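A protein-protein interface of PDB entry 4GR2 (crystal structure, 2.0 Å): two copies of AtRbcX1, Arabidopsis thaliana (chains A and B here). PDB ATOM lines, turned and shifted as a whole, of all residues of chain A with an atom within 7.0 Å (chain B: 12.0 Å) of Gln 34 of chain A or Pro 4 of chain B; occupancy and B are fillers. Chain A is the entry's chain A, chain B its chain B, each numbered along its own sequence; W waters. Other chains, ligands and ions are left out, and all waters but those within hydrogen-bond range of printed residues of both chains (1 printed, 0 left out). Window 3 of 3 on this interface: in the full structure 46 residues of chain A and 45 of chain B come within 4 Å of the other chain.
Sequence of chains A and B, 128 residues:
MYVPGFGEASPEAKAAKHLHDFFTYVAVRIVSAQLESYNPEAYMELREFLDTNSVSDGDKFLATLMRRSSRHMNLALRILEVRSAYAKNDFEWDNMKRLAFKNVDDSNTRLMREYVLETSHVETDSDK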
ATOM      1  N   VAL A  26      -4.138  20.542   5.232  1.00  0.00           N
ATOM      2  CA  VAL A  26      -3.962  20.767   6.660  1.00  0.00           C
ATOM      3  C   VAL A  26      -3.079  19.661   7.287  1.00  0.00           C
ATOM      4  O   VAL A  26      -2.137  19.940   8.047  1.00  0.00           O
ATOM      5  CB  VAL A  26      -5.340  20.851   7.355  1.00  0.00           C
ATOM      6  CG1 VAL A  26      -5.196  20.919   8.860  1.00  0.00           C
ATOM      7  CG2 VAL A  26      -6.085  22.070   6.850  1.00  0.00           C
ATOM      8  N   ALA A  27      -3.364  18.409   6.936  1.00  0.00           N
ATOM      9  CA  ALA A  27      -2.627  17.288   7.503  1.00  0.00           C
ATOM     10  C   ALA A  27      -1.150  17.390   7.156  1.00  0.00           C
ATOM     11  O   ALA A  27      -0.299  17.107   7.991  1.00  0.00           O
ATOM     12  CB  ALA A  27      -3.224  15.956   7.048  1.00  0.00           C
ATOM     13  N   VAL A  28      -0.830  17.825   5.940  1.00  0.00           N
ATOM     14  CA  VAL A  28       0.590  17.932   5.559  1.00  0.00           C
ATOM     15  C   VAL A  28       1.264  19.033   6.376  1.00  0.00           C
ATOM     16  O   VAL A  28       2.429  18.894   6.797  1.00  0.00           O
ATOM     17  CB  VAL A  28       0.790  18.131   4.028  1.00  0.00           C
ATOM     18  CG1 VAL A  28       2.236  18.499   3.688  1.00  0.00           C
ATOM     19  CG2 VAL A  28       0.426  16.850   3.293  1.00  0.00           C
ATOM     20  N   ARG A  29       0.504  20.096   6.643  1.00  0.00           N
ATOM     21  CA  ARG A  29       1.011  21.213   7.442  1.00  0.00           C
ATOM     22  C   ARG A  29       1.216  20.790   8.887  1.00  0.00           C
ATOM     23  O   ARG A  29       2.250  21.077   9.463  1.00  0.00           O
ATOM     24  CB  ARG A  29       0.118  22.477   7.335  1.00  0.00           C
ATOM     25  CG  ARG A  29       0.623  23.459   6.279  1.00  0.00           C
ATOM     26  CD  ARG A  29      -0.226  24.731   6.185  1.00  0.00           C
ATOM     27  NE  ARG A  29       0.125  25.785   7.147  1.00  0.00           N
ATOM     28  CZ  ARG A  29      -0.391  27.018   7.133  1.00  0.00           C
ATOM     29  NH1 ARG A  29      -1.276  27.363   6.204  1.00  0.00           N
ATOM     30  NH2 ARG A  29      -0.034  27.911   8.050  1.00  0.00           N
ATOM     31  N   ILE A  30       0.242  20.085   9.461  1.00  0.00           N
ATOM     32  CA  ILE A  30       0.393  19.556  10.811  1.00  0.00           C
ATOM     33  C   ILE A  30       1.579  18.590  10.926  1.00  0.00           C
ATOM     34  O   ILE A  30       2.410  18.690  11.830  1.00  0.00           O
ATOM     35  CB  ILE A  30      -0.876  18.817  11.238  1.00  0.00           C
ATOM     36  CG1 ILE A  30      -1.994  19.817  11.532  1.00  0.00           C
ATOM     37  CG2 ILE A  30      -0.586  17.901  12.419  1.00  0.00           C
ATOM     38  CD1 ILE A  30      -3.369  19.182  11.644  1.00  0.00           C
ATOM     39  N   VAL A  31       1.642  17.636  10.006  1.00  0.00           N
ATOM     40  CA  VAL A  31       2.699  16.645  10.020  1.00  0.00           C
ATOM     41  C   VAL A  31       4.067  17.295   9.855  1.00  0.00           C
ATOM     42  O   VAL A  31       5.044  16.905  10.519  1.00  0.00           O
ATOM     43  CB  VAL A  31       2.453  15.551   8.936  1.00  0.00           C
ATOM     44  CG1 VAL A  31       3.701  14.690   8.729  1.00  0.00           C
ATOM     45  CG2 VAL A  31       1.251  14.685   9.343  1.00  0.00           C
ATOM     46  N   SER A  32       4.152  18.273   8.961  1.00  0.00           N
ATOM     47  CA  SER A  32       5.418  18.976   8.734  1.00  0.00           C
ATOM     48  C   SER A  32       5.907  19.659  10.024  1.00  0.00           C
ATOM     49  O   SER A  32       7.063  19.502  10.412  1.00  0.00           O
ATOM     50  CB  SER A  32       5.274  20.012   7.616  1.00  0.00           C
ATOM     51  OG  SER A  32       6.545  20.494   7.232  1.00  0.00           O
ATOM     52  N   ALA A  33       5.004  20.405  10.659  1.00  0.00           N
ATOM     53  CA  ALA A  33       5.257  21.058  11.940  1.00  0.00           C
ATOM     54  C   ALA A  33       5.715  20.079  13.032  1.00  0.00           C
ATOM     55  O   ALA A  33       6.685  20.338  13.740  1.00  0.00           O
ATOM     56  CB  ALA A  33       4.010  21.824  12.395  1.00  0.00           C
ATOM     57  N   GLN A  34       5.035  18.943  13.164  1.00  0.00           N
ATOM     58  CA  GLN A  34       5.427  17.968  14.175  1.00  0.00           C
ATOM     59  C   GLN A  34       6.795  17.371  13.886  1.00  0.00           C
ATOM     60  O   GLN A  34       7.599  17.162  14.797  1.00  0.00           O
ATOM     61  CB  GLN A  34       4.354  16.878  14.327  1.00  0.00           C
ATOM     62  CG  GLN A  34       2.967  17.428  14.658  1.00  0.00           C
ATOM     63  CD  GLN A  34       2.809  17.828  16.135  1.00  0.00           C
ATOM     64  OE1 GLN A  34       3.683  18.463  16.721  1.00  0.00           O
ATOM     65  NE2 GLN A  34       1.685  17.446  16.733  1.00  0.00           N
ATOM     66  N   LEU A  35       7.068  17.088  12.619  1.00  0.00           N
ATOM     67  CA  LEU A  35       8.361  16.554  12.242  1.00  0.00           C
ATOM     68  C   LEU A  35       9.485  17.555  12.520  1.00  0.00           C
ATOM     69  O   LEU A  35      10.584  17.165  12.875  1.00  0.00           O
ATOM     70  CB  LEU A  35       8.383  16.146  10.765  1.00  0.00           C
ATOM     71  CG  LEU A  35       7.544  14.938  10.317  1.00  0.00           C
ATOM     72  CD1 LEU A  35       7.548  14.818   8.788  1.00  0.00           C
ATOM     73  CD2 LEU A  35       8.048  13.656  10.948  1.00  0.00           C
ATOM     74  N   GLU A  36       9.207  18.846  12.354  1.00  0.00           N
ATOM     75  CA  GLU A  36      10.222  19.865  12.639  1.00  0.00           C
ATOM     76  C   GLU A  36      10.708  19.751  14.090  1.00  0.00           C
ATOM     77  O   GLU A  36      11.902  19.776  14.330  1.00  0.00           O
ATOM     78  CB  GLU A  36       9.691  21.272  12.358  1.00  0.00           C
ATOM     79  CG  GLU A  36      10.764  22.276  11.954  1.00  0.00           C
ATOM     80  CD  GLU A  36      10.179  23.652  11.637  1.00  0.00           C
ATOM     81  OE1 GLU A  36       8.934  23.762  11.529  1.00  0.00           O
ATOM     82  OE2 GLU A  36      10.959  24.620  11.491  1.00  0.00           O
ATOM     83  N   SER A  37       9.772  19.583  15.031  1.00  0.00           N
ATOM     84  CA  SER A  37      10.082  19.369  16.449  1.00  0.00           C
ATOM     85  C   SER A  37      10.573  17.949  16.785  1.00  0.00           C
ATOM     86  O   SER A  37      11.475  17.781  17.615  1.00  0.00           O
ATOM     87  CB  SER A  37       8.860  19.673  17.338  1.00  0.00           C
ATOM     88  OG  SER A  37       8.251  20.912  17.036  1.00  0.00           O
ATOM     89  N   TYR A  38       9.980  16.927  16.167  1.00  0.00           N
ATOM     90  CA  TYR A  38      10.225  15.547  16.605  1.00  0.00           C
ATOM     91  C   TYR A  38      11.084  14.662  15.712  1.00  0.00           C
ATOM     92  O   TYR A  38      11.522  13.592  16.151  1.00  0.00           O
ATOM     93  CB  TYR A  38       8.907  14.842  16.909  1.00  0.00           C
ATOM     94  CG  TYR A  38       8.233  15.434  18.114  1.00  0.00           C
ATOM     95  CD1 TYR A  38       8.717  15.169  19.397  1.00  0.00           C
ATOM     96  CD2 TYR A  38       7.144  16.272  17.982  1.00  0.00           C
ATOM     97  CE1 TYR A  38       8.121  15.714  20.520  1.00  0.00           C
ATOM     98  CE2 TYR A  38       6.538  16.828  19.105  1.00  0.00           C
ATOM     99  CZ  TYR A  38       7.041  16.538  20.380  1.00  0.00           C
ATOM    100  OH  TYR A  38       6.444  17.099  21.498  1.00  0.00           O
ATOM    101  N   ASN A  39      11.323  15.090  14.472  1.00  0.00           N
ATOM    102  CA  ASN A  39      12.132  14.294  13.540  1.00  0.00           C
ATOM    103  C   ASN A  39      12.712  15.167  12.429  1.00  0.00           C
ATOM    104  O   ASN A  39      12.176  15.222  11.313  1.00  0.00           O
ATOM    105  CB  ASN A  39      11.289  13.161  12.940  1.00  0.00           C
ATOM    106  CG  ASN A  39      12.122  12.104  12.258  1.00  0.00           C
ATOM    107  OD1 ASN A  39      13.243  12.346  11.818  1.00  0.00           O
ATOM    108  ND2 ASN A  39      11.559  10.912  12.150  1.00  0.00           N
ATOM    109  N   PRO A  40      13.802  15.876  12.745  1.00  0.00           N
ATOM    110  CA  PRO A  40      14.518  16.758  11.817  1.00  0.00           C
ATOM    111  C   PRO A  40      14.829  16.143  10.439  1.00  0.00           C
ATOM    112  O   PRO A  40      14.554  16.786   9.430  1.00  0.00           O
ATOM    113  CB  PRO A  40      15.805  17.060  12.583  1.00  0.00           C
ATOM    114  CG  PRO A  40      15.346  17.078  14.017  1.00  0.00           C
ATOM    115  CD  PRO A  40      14.350  15.962  14.114  1.00  0.00           C
ATOM    116  N   TYR A  43      11.521  15.603   8.567  1.00  0.00           N
ATOM    117  CA  TYR A  43      11.116  16.940   8.174  1.00  0.00           C
ATOM    118  C   TYR A  43      11.747  17.395   6.845  1.00  0.00           C
ATOM    119  O   TYR A  43      11.059  17.959   5.978  1.00  0.00           O
ATOM    120  CB  TYR A  43      11.438  17.941   9.285  1.00  0.00           C
ATOM    121  CG  TYR A  43      11.275  19.371   8.835  1.00  0.00           C
ATOM    122  CD1 TYR A  43      10.018  19.941   8.733  1.00  0.00           C
ATOM    123  CD2 TYR A  43      12.380  20.134   8.464  1.00  0.00           C
ATOM    124  CE1 TYR A  43       9.851  21.245   8.308  1.00  0.00           C
ATOM    125  CE2 TYR A  43      12.227  21.447   8.040  1.00  0.00           C
ATOM    126  CZ  TYR A  43      10.962  21.996   7.968  1.00  0.00           C
ATOM    127  OH  TYR A  43      10.794  23.287   7.544  1.00  0.00           O
ATOM    128  N   VAL A  82      -3.349  11.451  10.233  1.00  0.00           N
ATOM    129  CA  VAL A  82      -3.585  12.795  10.751  1.00  0.00           C
ATOM    130  C   VAL A  82      -4.767  13.442  10.036  1.00  0.00           C
ATOM    131  O   VAL A  82      -5.617  14.067  10.656  1.00  0.00           O
ATOM    132  CB  VAL A  82      -2.297  13.666  10.667  1.00  0.00           C
ATOM    133  CG1 VAL A  82      -2.604  15.185  10.926  1.00  0.00           C
ATOM    134  CG2 VAL A  82      -1.244  13.139  11.642  1.00  0.00           C
ATOM    135  N   TYR A  86      -7.832  14.601  12.346  1.00  0.00           N
ATOM    136  CA  TYR A  86      -8.064  16.044  12.381  1.00  0.00           C
ATOM    137  C   TYR A  86      -9.487  16.434  11.958  1.00  0.00           C
ATOM    138  O   TYR A  86     -10.187  17.189  12.665  1.00  0.00           O
ATOM    139  CB  TYR A  86      -7.054  16.807  11.514  1.00  0.00           C
ATOM    140  CG  TYR A  86      -7.342  18.290  11.547  1.00  0.00           C
ATOM    141  CD1 TYR A  86      -7.017  19.037  12.668  1.00  0.00           C
ATOM    142  CD2 TYR A  86      -7.969  18.935  10.477  1.00  0.00           C
ATOM    143  CE1 TYR A  86      -7.303  20.395  12.734  1.00  0.00           C
ATOM    144  CE2 TYR A  86      -8.252  20.305  10.527  1.00  0.00           C
ATOM    145  CZ  TYR A  86      -7.920  21.020  11.664  1.00  0.00           C
ATOM    146  OH  TYR A  86      -8.188  22.362  11.753  1.00  0.00           O
ATOM    147  N   VAL B   3      -3.399  24.562  16.501  1.00  0.00           N
ATOM    148  CA  VAL B   3      -3.183  23.563  15.453  1.00  0.00           C
ATOM    149  C   VAL B   3      -1.775  23.692  14.859  1.00  0.00           C
ATOM    150  O   VAL B   3      -1.420  24.737  14.306  1.00  0.00           O
ATOM    151  CB  VAL B   3      -4.250  23.644  14.321  1.00  0.00           C
ATOM    152  CG1 VAL B   3      -4.041  22.526  13.325  1.00  0.00           C
ATOM    153  CG2 VAL B   3      -5.663  23.563  14.879  1.00  0.00           C
ATOM    154  N   PRO B   4      -0.961  22.628  14.991  1.00  0.00           N
ATOM    155  CA  PRO B   4       0.426  22.660  14.503  1.00  0.00           C
ATOM    156  C   PRO B   4       0.543  23.137  13.054  1.00  0.00           C
ATOM    157  O   PRO B   4      -0.180  22.654  12.180  1.00  0.00           O
ATOM    158  CB  PRO B   4       0.877  21.198  14.641  1.00  0.00           C
ATOM    159  CG  PRO B   4       0.064  20.690  15.817  1.00  0.00           C
ATOM    160  CD  PRO B   4      -1.273  21.369  15.698  1.00  0.00           C
ATOM    161  N   GLY B   5       1.419  24.109  12.813  1.00  0.00           N
ATOM    162  CA  GLY B   5       1.662  24.586  11.464  1.00  0.00           C
ATOM    163  C   GLY B   5       0.780  25.733  11.024  1.00  0.00           C
ATOM    164  O   GLY B   5       0.938  26.233   9.905  1.00  0.00           O
ATOM    165  N   PHE B   6      -0.145  26.130  11.903  1.00  0.00           N
ATOM    166  CA  PHE B   6      -1.056  27.268  11.691  1.00  0.00           C
ATOM    167  C   PHE B   6      -0.888  28.335  12.786  1.00  0.00           C
ATOM    168  O   PHE B   6      -1.062  28.056  13.976  1.00  0.00           O
ATOM    169  CB  PHE B   6      -2.523  26.792  11.632  1.00  0.00           C
ATOM    170  CG  PHE B   6      -2.851  25.992  10.392  1.00  0.00           C
ATOM    171  CD1 PHE B   6      -2.577  24.626  10.339  1.00  0.00           C
ATOM    172  CD2 PHE B   6      -3.408  26.608   9.274  1.00  0.00           C
ATOM    173  CE1 PHE B   6      -2.853  23.897   9.197  1.00  0.00           C
ATOM    174  CE2 PHE B   6      -3.689  25.881   8.126  1.00  0.00           C
ATOM    175  CZ  PHE B   6      -3.417  24.531   8.084  1.00  0.00           C
ATOM    176  N   GLY B   7      -0.554  29.554  12.374  1.00  0.00           N
ATOM    177  CA  GLY B   7      -0.369  30.644  13.313  1.00  0.00           C
ATOM    178  C   GLY B   7      -0.880  31.972  12.788  1.00  0.00           C
ATOM    179  O   GLY B   7      -0.468  33.037  13.255  1.00  0.00           O
ATOM    180  N   GLU B   8      -1.775  31.905  11.807  1.00  0.00           N
ATOM    181  CA  GLU B   8      -2.405  33.095  11.245  1.00  0.00           C
ATOM    182  C   GLU B   8      -3.921  32.917  11.286  1.00  0.00           C
ATOM    183  O   GLU B   8      -4.551  33.047  12.338  1.00  0.00           O
ATOM    184  CB  GLU B   8      -1.925  33.328   9.809  1.00  0.00           C
ATOM    185  N   ALA B   9      -4.503  32.618  10.133  1.00  0.00           N
ATOM    186  CA  ALA B   9      -5.895  32.206  10.074  1.00  0.00           C
ATOM    187  C   ALA B   9      -5.999  30.743  10.510  1.00  0.00           C
ATOM    188  O   ALA B   9      -5.128  29.932  10.194  1.00  0.00           O
ATOM    189  CB  ALA B   9      -6.430  32.380   8.672  1.00  0.00           C
ATOM    190  N   SER B  10      -7.047  30.411  11.262  1.00  0.00           N
ATOM    191  CA  SER B  10      -7.337  29.016  11.589  1.00  0.00           C
ATOM    192  C   SER B  10      -7.754  28.291  10.311  1.00  0.00           C
ATOM    193  O   SER B  10      -8.136  28.941   9.330  1.00  0.00           O
ATOM    194  CB  SER B  10      -8.510  28.952  12.566  1.00  0.00           C
ATOM    195  OG  SER B  10      -9.682  29.437  11.921  1.00  0.00           O
ATOM    196  N   PRO B  11      -7.697  26.947  10.316  1.00  0.00           N
ATOM    197  CA  PRO B  11      -8.291  26.211   9.197  1.00  0.00           C
ATOM    198  C   PRO B  11      -9.781  26.500   9.068  1.00  0.00           C
ATOM    199  O   PRO B  11     -10.285  26.539   7.950  1.00  0.00           O
ATOM    200  CB  PRO B  11      -8.063  24.752   9.583  1.00  0.00           C
ATOM    201  CG  PRO B  11      -6.799  24.786  10.414  1.00  0.00           C
ATOM    202  CD  PRO B  11      -6.904  26.064  11.200  1.00  0.00           C
ATOM    203  N   GLU B  12     -10.477  26.693  10.190  1.00  0.00           N
ATOM    204  CA  GLU B  12     -11.905  27.010  10.139  1.00  0.00           C
ATOM    205  C   GLU B  12     -12.175  28.336   9.422  1.00  0.00           C
ATOM    206  O   GLU B  12     -13.118  28.450   8.609  1.00  0.00           O
ATOM    207  CB  GLU B  12     -12.478  27.024  11.548  1.00  0.00           C
ATOM    208  CG  GLU B  12     -12.512  25.642  12.189  1.00  0.00           C
ATOM    209  CD  GLU B  12     -11.244  25.270  12.934  1.00  0.00           C
ATOM    210  OE1 GLU B  12     -10.266  26.057  12.925  1.00  0.00           O
ATOM    211  OE2 GLU B  12     -11.238  24.174  13.554  1.00  0.00           O
ATOM    212  N   LYS B  14     -10.212  29.784   7.291  1.00  0.00           N
ATOM    213  CA  LYS B  14      -9.860  29.586   5.888  1.00  0.00           C
ATOM    214  C   LYS B  14     -11.000  28.918   5.140  1.00  0.00           C
ATOM    215  O   LYS B  14     -11.388  29.367   4.061  1.00  0.00           O
ATOM    216  CB  LYS B  14      -8.559  28.772   5.748  1.00  0.00           C
ATOM    217  CG  LYS B  14      -7.293  29.531   6.201  1.00  0.00           C
ATOM    218  CD  LYS B  14      -6.142  28.575   6.545  1.00  0.00           C
ATOM    219  CE  LYS B  14      -4.881  28.827   5.727  1.00  0.00           C
ATOM    220  NZ  LYS B  14      -4.260  30.145   6.039  1.00  0.00           N
HETATM  221  O   HOH W   1      -8.876  23.143  14.481  1.00  0.00           O
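O of Gly 5 of chain B lies within hydrogen-bond range of NH2 of Arg 29 of chain A, at 2.7 Å.
The side-chain hydroxyl (OG) of Ser 10 of chain B lies close to the backbone NH (N) of Glu 12 of chain B, at 3.3 Å.
Among the printed residues, pairs that only touch across the chains: Tyr 86 of chain A with Pro 11 of chain B (3.1 Å), Arg 29 of chain A with Phe 6 of chain B (3.4 Å), Ile 30 of chain A with Pro 4 of chain B (3.4 Å), Ala 33 of chain A with Gly 5 of chain B (3.5 Å), Gln 34 of chain A with Pro 4 of chain B (3.7 Å), Ala 33 of chain A with Pro 4 of chain B (3.8 Å), Ile 30 of chain A with Val 3 of chain B (3.8 Å), Val 26 of chain A with Phe 6 of chain B (3.8 Å), Arg 29 of chain A with Lys 14 of chain B (3.9 Å), Tyr 86 of chain A with Val 3 of chain B (3.9 Å), Arg 29 of chain A with Pro 4 of chain B (3.97 Å) and Tyr 86 of chain A with Glu 12 of chain B (3.98 Å).
Of chain B, only Pro 4 (3.97 Å), Gly 5 (2.7 Å), Phe 6 (3.4 Å) and Lys 14 (3.9 Å) come within 4 Å of Arg 29 of chain A.
Of chain B, only Pro 4 (3.8 Å) and Gly 5 (3.5 Å) come within 4 Å of Ala 33 of chain A.
Gln 34 of chain A touches one residue of chain B.
Leu 35 of chain A touches none of the printed residues of chain B.
Of the printed residues of chain A, Val 3 of chain B touches Ile 30 and Tyr 86.
Pro 4 of chain B touches just these residues of chain A: Arg 29, Ile 30, Ala 33 and Gln 34.
Printed residues of chain A within 4 Å of Gly 5 of chain B: Arg 29 (2.7 Å) and Ala 33 (3.5 Å).
Of the printed residues of chain A, Phe 6 of chain B touches Val 26 and Arg 29.
Glu 8 of chain B touches none of the printed residues of chain A.
Of the printed residues of chain A, Glu 12 of chain B touches Tyr 86.
Printed residues of chain A within 4 Å of Lys 14 of chain B: Arg 29.
The nearest residue of chain A that does not touch Pro 4 of chain B is Val 26 of chain A (5.3 Å).
The nearest printed residue of chain A that does not touch Gly 5 of chain B is Ile 30 of chain A (5.1 Å).
Printed residues of chain A that touch a printed residue of chain B: Val 26, Arg 29, Ile 30, Ala 33, Gln 34 and Tyr 86.
Along chain A the printed residues that touch a printed residue of chain B span positions 26 to 86.
Along chain B the printed residues that touch a printed residue of chain A span positions 3 to 14.
No position is printed for both chains.
Water W1 bridges OE2 of Glu 12 of chain B and OH of Tyr 86 of chain A.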
